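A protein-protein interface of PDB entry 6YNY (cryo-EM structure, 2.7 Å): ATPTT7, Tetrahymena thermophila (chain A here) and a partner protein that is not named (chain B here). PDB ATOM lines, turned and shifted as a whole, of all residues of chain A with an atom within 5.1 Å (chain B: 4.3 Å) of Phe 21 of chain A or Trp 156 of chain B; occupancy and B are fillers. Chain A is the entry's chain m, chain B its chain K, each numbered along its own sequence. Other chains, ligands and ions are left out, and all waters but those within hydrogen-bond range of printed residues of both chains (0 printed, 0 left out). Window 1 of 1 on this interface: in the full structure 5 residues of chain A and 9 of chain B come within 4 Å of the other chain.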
ATOM      1  N   PRO A  19      34.090 -20.255  22.115  1.00  0.00           N
ATOM      2  CA  PRO A  19      33.146 -20.873  23.037  1.00  0.00           C
ATOM      3  C   PRO A  19      32.579 -22.151  22.449  1.00  0.00           C
ATOM      4  O   PRO A  19      32.328 -22.226  21.237  1.00  0.00           O
ATOM      5  CB  PRO A  19      32.062 -19.799  23.209  1.00  0.00           C
ATOM      6  CG  PRO A  19      32.209 -18.913  22.037  1.00  0.00           C
ATOM      7  CD  PRO A  19      33.653 -18.911  21.705  1.00  0.00           C
ATOM      8  N   PRO A  20      32.360 -23.179  23.267  1.00  0.00           N
ATOM      9  CA  PRO A  20      31.924 -24.476  22.742  1.00  0.00           C
ATOM     10  C   PRO A  20      30.448 -24.561  22.386  1.00  0.00           C
ATOM     11  O   PRO A  20      29.964 -25.662  22.116  1.00  0.00           O
ATOM     12  CB  PRO A  20      32.257 -25.426  23.900  1.00  0.00           C
ATOM     13  CG  PRO A  20      32.127 -24.596  25.105  1.00  0.00           C
ATOM     14  CD  PRO A  20      32.544 -23.212  24.727  1.00  0.00           C
ATOM     15  N   PHE A  21      29.725 -23.447  22.376  1.00  0.00           N
ATOM     16  CA  PHE A  21      28.300 -23.433  22.077  1.00  0.00           C
ATOM     17  C   PHE A  21      28.042 -22.575  20.848  1.00  0.00           C
ATOM     18  O   PHE A  21      28.664 -21.524  20.669  1.00  0.00           O
ATOM     19  CB  PHE A  21      27.507 -22.929  23.274  1.00  0.00           C
ATOM     20  CG  PHE A  21      27.738 -23.731  24.517  1.00  0.00           C
ATOM     21  CD1 PHE A  21      27.136 -24.962  24.682  1.00  0.00           C
ATOM     22  CD2 PHE A  21      28.572 -23.264  25.512  1.00  0.00           C
ATOM     23  CE1 PHE A  21      27.356 -25.705  25.815  1.00  0.00           C
ATOM     24  CE2 PHE A  21      28.792 -24.004  26.647  1.00  0.00           C
ATOM     25  CZ  PHE A  21      28.186 -25.223  26.799  1.00  0.00           C
ATOM     26  N   LYS A  22      27.110 -23.029  20.009  1.00  0.00           N
ATOM     27  CA  LYS A  22      26.890 -22.384  18.719  1.00  0.00           C
ATOM     28  C   LYS A  22      26.379 -20.959  18.873  1.00  0.00           C
ATOM     29  O   LYS A  22      26.746 -20.076  18.089  1.00  0.00           O
ATOM     30  CB  LYS A  22      25.902 -23.197  17.888  1.00  0.00           C
ATOM     31  CG  LYS A  22      26.450 -24.475  17.311  1.00  0.00           C
ATOM     32  CD  LYS A  22      25.360 -25.212  16.568  1.00  0.00           C
ATOM     33  CE  LYS A  22      25.886 -26.418  15.829  1.00  0.00           C
ATOM     34  NZ  LYS A  22      24.771 -27.230  15.273  1.00  0.00           N
ATOM     35  N   ASP A  23      25.530 -20.710  19.868  1.00  0.00           N
ATOM     36  CA  ASP A  23      24.926 -19.389  20.003  1.00  0.00           C
ATOM     37  C   ASP A  23      25.994 -18.306  20.097  1.00  0.00           C
ATOM     38  O   ASP A  23      26.030 -17.378  19.282  1.00  0.00           O
ATOM     39  CB  ASP A  23      24.014 -19.356  21.228  1.00  0.00           C
ATOM     40  CG  ASP A  23      23.145 -18.120  21.270  1.00  0.00           C
ATOM     41  OD1 ASP A  23      23.188 -17.326  20.309  1.00  0.00           O
ATOM     42  OD2 ASP A  23      22.415 -17.941  22.267  1.00  0.00           O
ATOM     43  N   ALA A  24      26.885 -18.418  21.079  1.00  0.00           N
ATOM     44  CA  ALA A  24      27.931 -17.416  21.235  1.00  0.00           C
ATOM     45  C   ALA A  24      28.996 -17.539  20.157  1.00  0.00           C
ATOM     46  O   ALA A  24      29.634 -16.542  19.800  1.00  0.00           O
ATOM     47  CB  ALA A  24      28.567 -17.540  22.613  1.00  0.00           C
ATOM     48  N   ARG A  25      29.204 -18.743  19.630  1.00  0.00           N
ATOM     49  CA  ARG A  25      30.241 -18.941  18.626  1.00  0.00           C
ATOM     50  C   ARG A  25      29.859 -18.287  17.306  1.00  0.00           C
ATOM     51  O   ARG A  25      30.712 -17.717  16.617  1.00  0.00           O
ATOM     52  CB  ARG A  25      30.491 -20.432  18.440  1.00  0.00           C
ATOM     53  CG  ARG A  25      31.759 -20.783  17.703  1.00  0.00           C
ATOM     54  CD  ARG A  25      31.687 -22.205  17.214  1.00  0.00           C
ATOM     55  NE  ARG A  25      31.336 -23.124  18.288  1.00  0.00           N
ATOM     56  CZ  ARG A  25      30.785 -24.317  18.104  1.00  0.00           C
ATOM     57  NH1 ARG A  25      30.507 -24.742  16.884  1.00  0.00           N
ATOM     58  NH2 ARG A  25      30.500 -25.082  19.143  1.00  0.00           N
ATOM     59  N   LEU A  26      28.581 -18.359  16.937  1.00  0.00           N
ATOM     60  CA  LEU A  26      28.129 -17.760  15.688  1.00  0.00           C
ATOM     61  C   LEU A  26      28.002 -16.247  15.793  1.00  0.00           C
ATOM     62  O   LEU A  26      28.165 -15.548  14.787  1.00  0.00           O
ATOM     63  CB  LEU A  26      26.795 -18.372  15.267  1.00  0.00           C
ATOM     64  CG  LEU A  26      26.865 -19.638  14.406  1.00  0.00           C
ATOM     65  CD1 LEU A  26      27.662 -20.740  15.073  1.00  0.00           C
ATOM     66  CD2 LEU A  26      25.469 -20.127  14.080  1.00  0.00           C
ATOM     67  N   ARG B 106      22.834 -28.878  32.716  1.00  0.00           N
ATOM     68  CA  ARG B 106      22.359 -27.657  32.080  1.00  0.00           C
ATOM     69  C   ARG B 106      21.330 -27.941  30.996  1.00  0.00           C
ATOM     70  O   ARG B 106      20.568 -27.040  30.629  1.00  0.00           O
ATOM     71  CB  ARG B 106      23.546 -26.882  31.525  1.00  0.00           C
ATOM     72  CG  ARG B 106      24.403 -26.277  32.617  1.00  0.00           C
ATOM     73  CD  ARG B 106      25.665 -25.644  32.080  1.00  0.00           C
ATOM     74  NE  ARG B 106      26.593 -26.629  31.543  1.00  0.00           N
ATOM     75  CZ  ARG B 106      27.790 -26.329  31.058  1.00  0.00           C
ATOM     76  NH1 ARG B 106      28.574 -27.287  30.591  1.00  0.00           N
ATOM     77  NH2 ARG B 106      28.202 -25.071  31.039  1.00  0.00           N
ATOM     78  N   VAL B 145      30.036 -31.621  22.298  1.00  0.00           N
ATOM     79  CA  VAL B 145      30.238 -30.591  23.312  1.00  0.00           C
ATOM     80  C   VAL B 145      30.790 -31.211  24.588  1.00  0.00           C
ATOM     81  O   VAL B 145      31.787 -30.743  25.148  1.00  0.00           O
ATOM     82  CB  VAL B 145      28.924 -29.839  23.581  1.00  0.00           C
ATOM     83  CG1 VAL B 145      29.114 -28.830  24.685  1.00  0.00           C
ATOM     84  CG2 VAL B 145      28.430 -29.165  22.325  1.00  0.00           C
ATOM     85  N   ASP B 154      34.710 -25.211  28.481  1.00  0.00           N
ATOM     86  CA  ASP B 154      33.337 -25.072  28.931  1.00  0.00           C
ATOM     87  C   ASP B 154      33.066 -23.598  29.179  1.00  0.00           C
ATOM     88  O   ASP B 154      33.988 -22.794  29.329  1.00  0.00           O
ATOM     89  CB  ASP B 154      33.067 -25.896  30.190  1.00  0.00           C
ATOM     90  CG  ASP B 154      31.598 -25.973  30.531  1.00  0.00           C
ATOM     91  OD1 ASP B 154      30.786 -25.367  29.803  1.00  0.00           O
ATOM     92  OD2 ASP B 154      31.251 -26.646  31.523  1.00  0.00           O
ATOM     93  N   SER B 155      31.787 -23.251  29.214  1.00  0.00           N
ATOM     94  CA  SER B 155      31.373 -21.872  29.408  1.00  0.00           C
ATOM     95  C   SER B 155      29.920 -21.871  29.855  1.00  0.00           C
ATOM     96  O   SER B 155      29.351 -22.916  30.187  1.00  0.00           O
ATOM     97  CB  SER B 155      31.574 -21.059  28.128  1.00  0.00           C
ATOM     98  OG  SER B 155      31.230 -19.702  28.327  1.00  0.00           O
ATOM     99  N   TRP B 156      29.320 -20.689  29.871  1.00  0.00           N
ATOM    100  CA  TRP B 156      27.922 -20.555  30.232  1.00  0.00           C
ATOM    101  C   TRP B 156      27.039 -20.842  29.026  1.00  0.00           C
ATOM    102  O   TRP B 156      27.457 -20.698  27.874  1.00  0.00           O
ATOM    103  CB  TRP B 156      27.640 -19.155  30.775  1.00  0.00           C
ATOM    104  CG  TRP B 156      27.975 -18.064  29.820  1.00  0.00           C
ATOM    105  CD1 TRP B 156      29.165 -17.418  29.706  1.00  0.00           C
ATOM    106  CD2 TRP B 156      27.110 -17.489  28.839  1.00  0.00           C
ATOM    107  NE1 TRP B 156      29.099 -16.474  28.716  1.00  0.00           N
ATOM    108  CE2 TRP B 156      27.846 -16.497  28.168  1.00  0.00           C
ATOM    109  CE3 TRP B 156      25.784 -17.714  28.464  1.00  0.00           C
ATOM    110  CZ2 TRP B 156      27.302 -15.734  27.143  1.00  0.00           C
ATOM    111  CZ3 TRP B 156      25.247 -16.954  27.451  1.00  0.00           C
ATOM    112  CH2 TRP B 156      26.004 -15.977  26.800  1.00  0.00           C
ATOM    113  N   MET B 157      25.811 -21.261  29.303  1.00  0.00           N
ATOM    114  CA  MET B 157      24.853 -21.629  28.275  1.00  0.00           C
ATOM    115  C   MET B 157      23.664 -20.685  28.311  1.00  0.00           C
ATOM    116  O   MET B 157      23.185 -20.313  29.386  1.00  0.00           O
ATOM    117  CB  MET B 157      24.380 -23.068  28.467  1.00  0.00           C
ATOM    118  CG  MET B 157      25.474 -24.091  28.296  1.00  0.00           C
ATOM    119  SD  MET B 157      24.961 -25.768  28.690  1.00  0.00           S
ATOM    120  CE  MET B 157      23.699 -26.012  27.455  1.00  0.00           C
ATOM    121  N   SER B 158      23.196 -20.298  27.129  1.00  0.00           N
ATOM    122  CA  SER B 158      22.017 -19.460  27.012  1.00  0.00           C
ATOM    123  C   SER B 158      20.758 -20.316  27.095  1.00  0.00           C
ATOM    124  O   SER B 158      20.808 -21.546  27.173  1.00  0.00           O
ATOM    125  CB  SER B 158      22.058 -18.677  25.705  1.00  0.00           C
ATOM    126  OG  SER B 158      22.119 -19.548  24.593  1.00  0.00           O
ATOM    127  N   ASP B 161      20.736 -22.539  23.965  1.00  0.00           N
ATOM    128  CA  ASP B 161      21.650 -23.669  24.051  1.00  0.00           C
ATOM    129  C   ASP B 161      21.142 -24.719  25.028  1.00  0.00           C
ATOM    130  O   ASP B 161      21.340 -25.918  24.806  1.00  0.00           O
ATOM    131  CB  ASP B 161      23.039 -23.193  24.474  1.00  0.00           C
ATOM    132  CG  ASP B 161      23.686 -22.291  23.448  1.00  0.00           C
ATOM    133  OD1 ASP B 161      23.424 -22.474  22.242  1.00  0.00           O
ATOM    134  OD2 ASP B 161      24.462 -21.400  23.849  1.00  0.00           O
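Pro 20 of chain A touches Val 145 of chain B. Phe 21 of chain A touches Val 145 of chain B. CE2 of Phe 21 of chain A touches OD1 of Asp 154 of chain B, at 3.97 Å. Phe 21 of chain A touches Ser 155 of chain B (CE2 to O, 3.7 Å). Trp 156 of chain B touches Phe 21 of chain A (O to CD2, 3.7 Å). Met 157 of chain B touches Phe 21 of chain A. OD2 of Asp 161 of chain B touches CB of Phe 21 of chain A, at 3.5 Å. OD1 of Asp 161 of chain B touches CB of Asp 23 of chain A, at 3.3 Å.
The side-chain hydroxyl (OG) of Ser 158 of chain B is in hydrogen-bond range of the side-chain carboxylate (OD2) of Asp 161 of chain B (3.1 Å). The guanidinium group (NH2) of Arg 106 of chain B lies within hydrogen-bond range of the backbone carbonyl oxygen (O) of Ser 155 of chain B, 2.6 Å away. The side-chain sulfur (SD) of Met 157 of chain B lies close to the guanidinium group (NE) of Arg 106 of chain B (3.4 Å). OD1 of Asp 154 of chain B is in salt-bridge range of NH2 of Arg 106 of chain B (2.9 Å). The backbone carbonyl oxygen (O) of Pro 20 of chain A sits at hydrogen-bond distance from the guanidinium group (NH2) of Arg 25 of chain A, 3.1 Å away.
Of the 8 printed residues of chain B, 7 touch a printed residue of chain A. Hydrophobic or aromatic side chains of chain B within 4 Å of the printed part of chain A: Val 145 and Met 157. Among the printed residues, 9 pairs touch across the chains.
Of the printed residues of chain B, Pro 20 of chain A touches Val 145 (3.8 Å). Of chain B, only Val 145 (3.8 Å), Asp 154 (3.97 Å), Ser 155 (3.7 Å), Trp 156 (3.7 Å), Met 157 (3.3 Å) and Asp 161 (3.5 Å) come within 4 Å of Phe 21 of chain A. Lys 22 of chain A touches none of the printed residues of chain B. Of the printed residues of chain B, Asp 23 of chain A touches Ser 158 and Asp 161. Leu 26 of chain A touches none of the printed residues of chain B. Printed residues of chain A within 4 Å of Val 145 of chain B: Pro 20 and Phe 21. Of the printed residues of chain A, Ser 155 of chain B touches Phe 21 (3.7 Å). Of chain A, only Phe 21 (3.7 Å) comes within 4 Å of Trp 156 of chain B. Of the printed residues of chain A, Ser 158 of chain B touches Asp 23. The nearest residue of chain B that does not touch Phe 21 of chain A is Arg 106 of chain B (4.2 Å).
The side-chain carboxylate of Asp 23 of chain A lies within hydrogen-bond range of the side-chain hydroxyl of Ser 158 of chain B.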
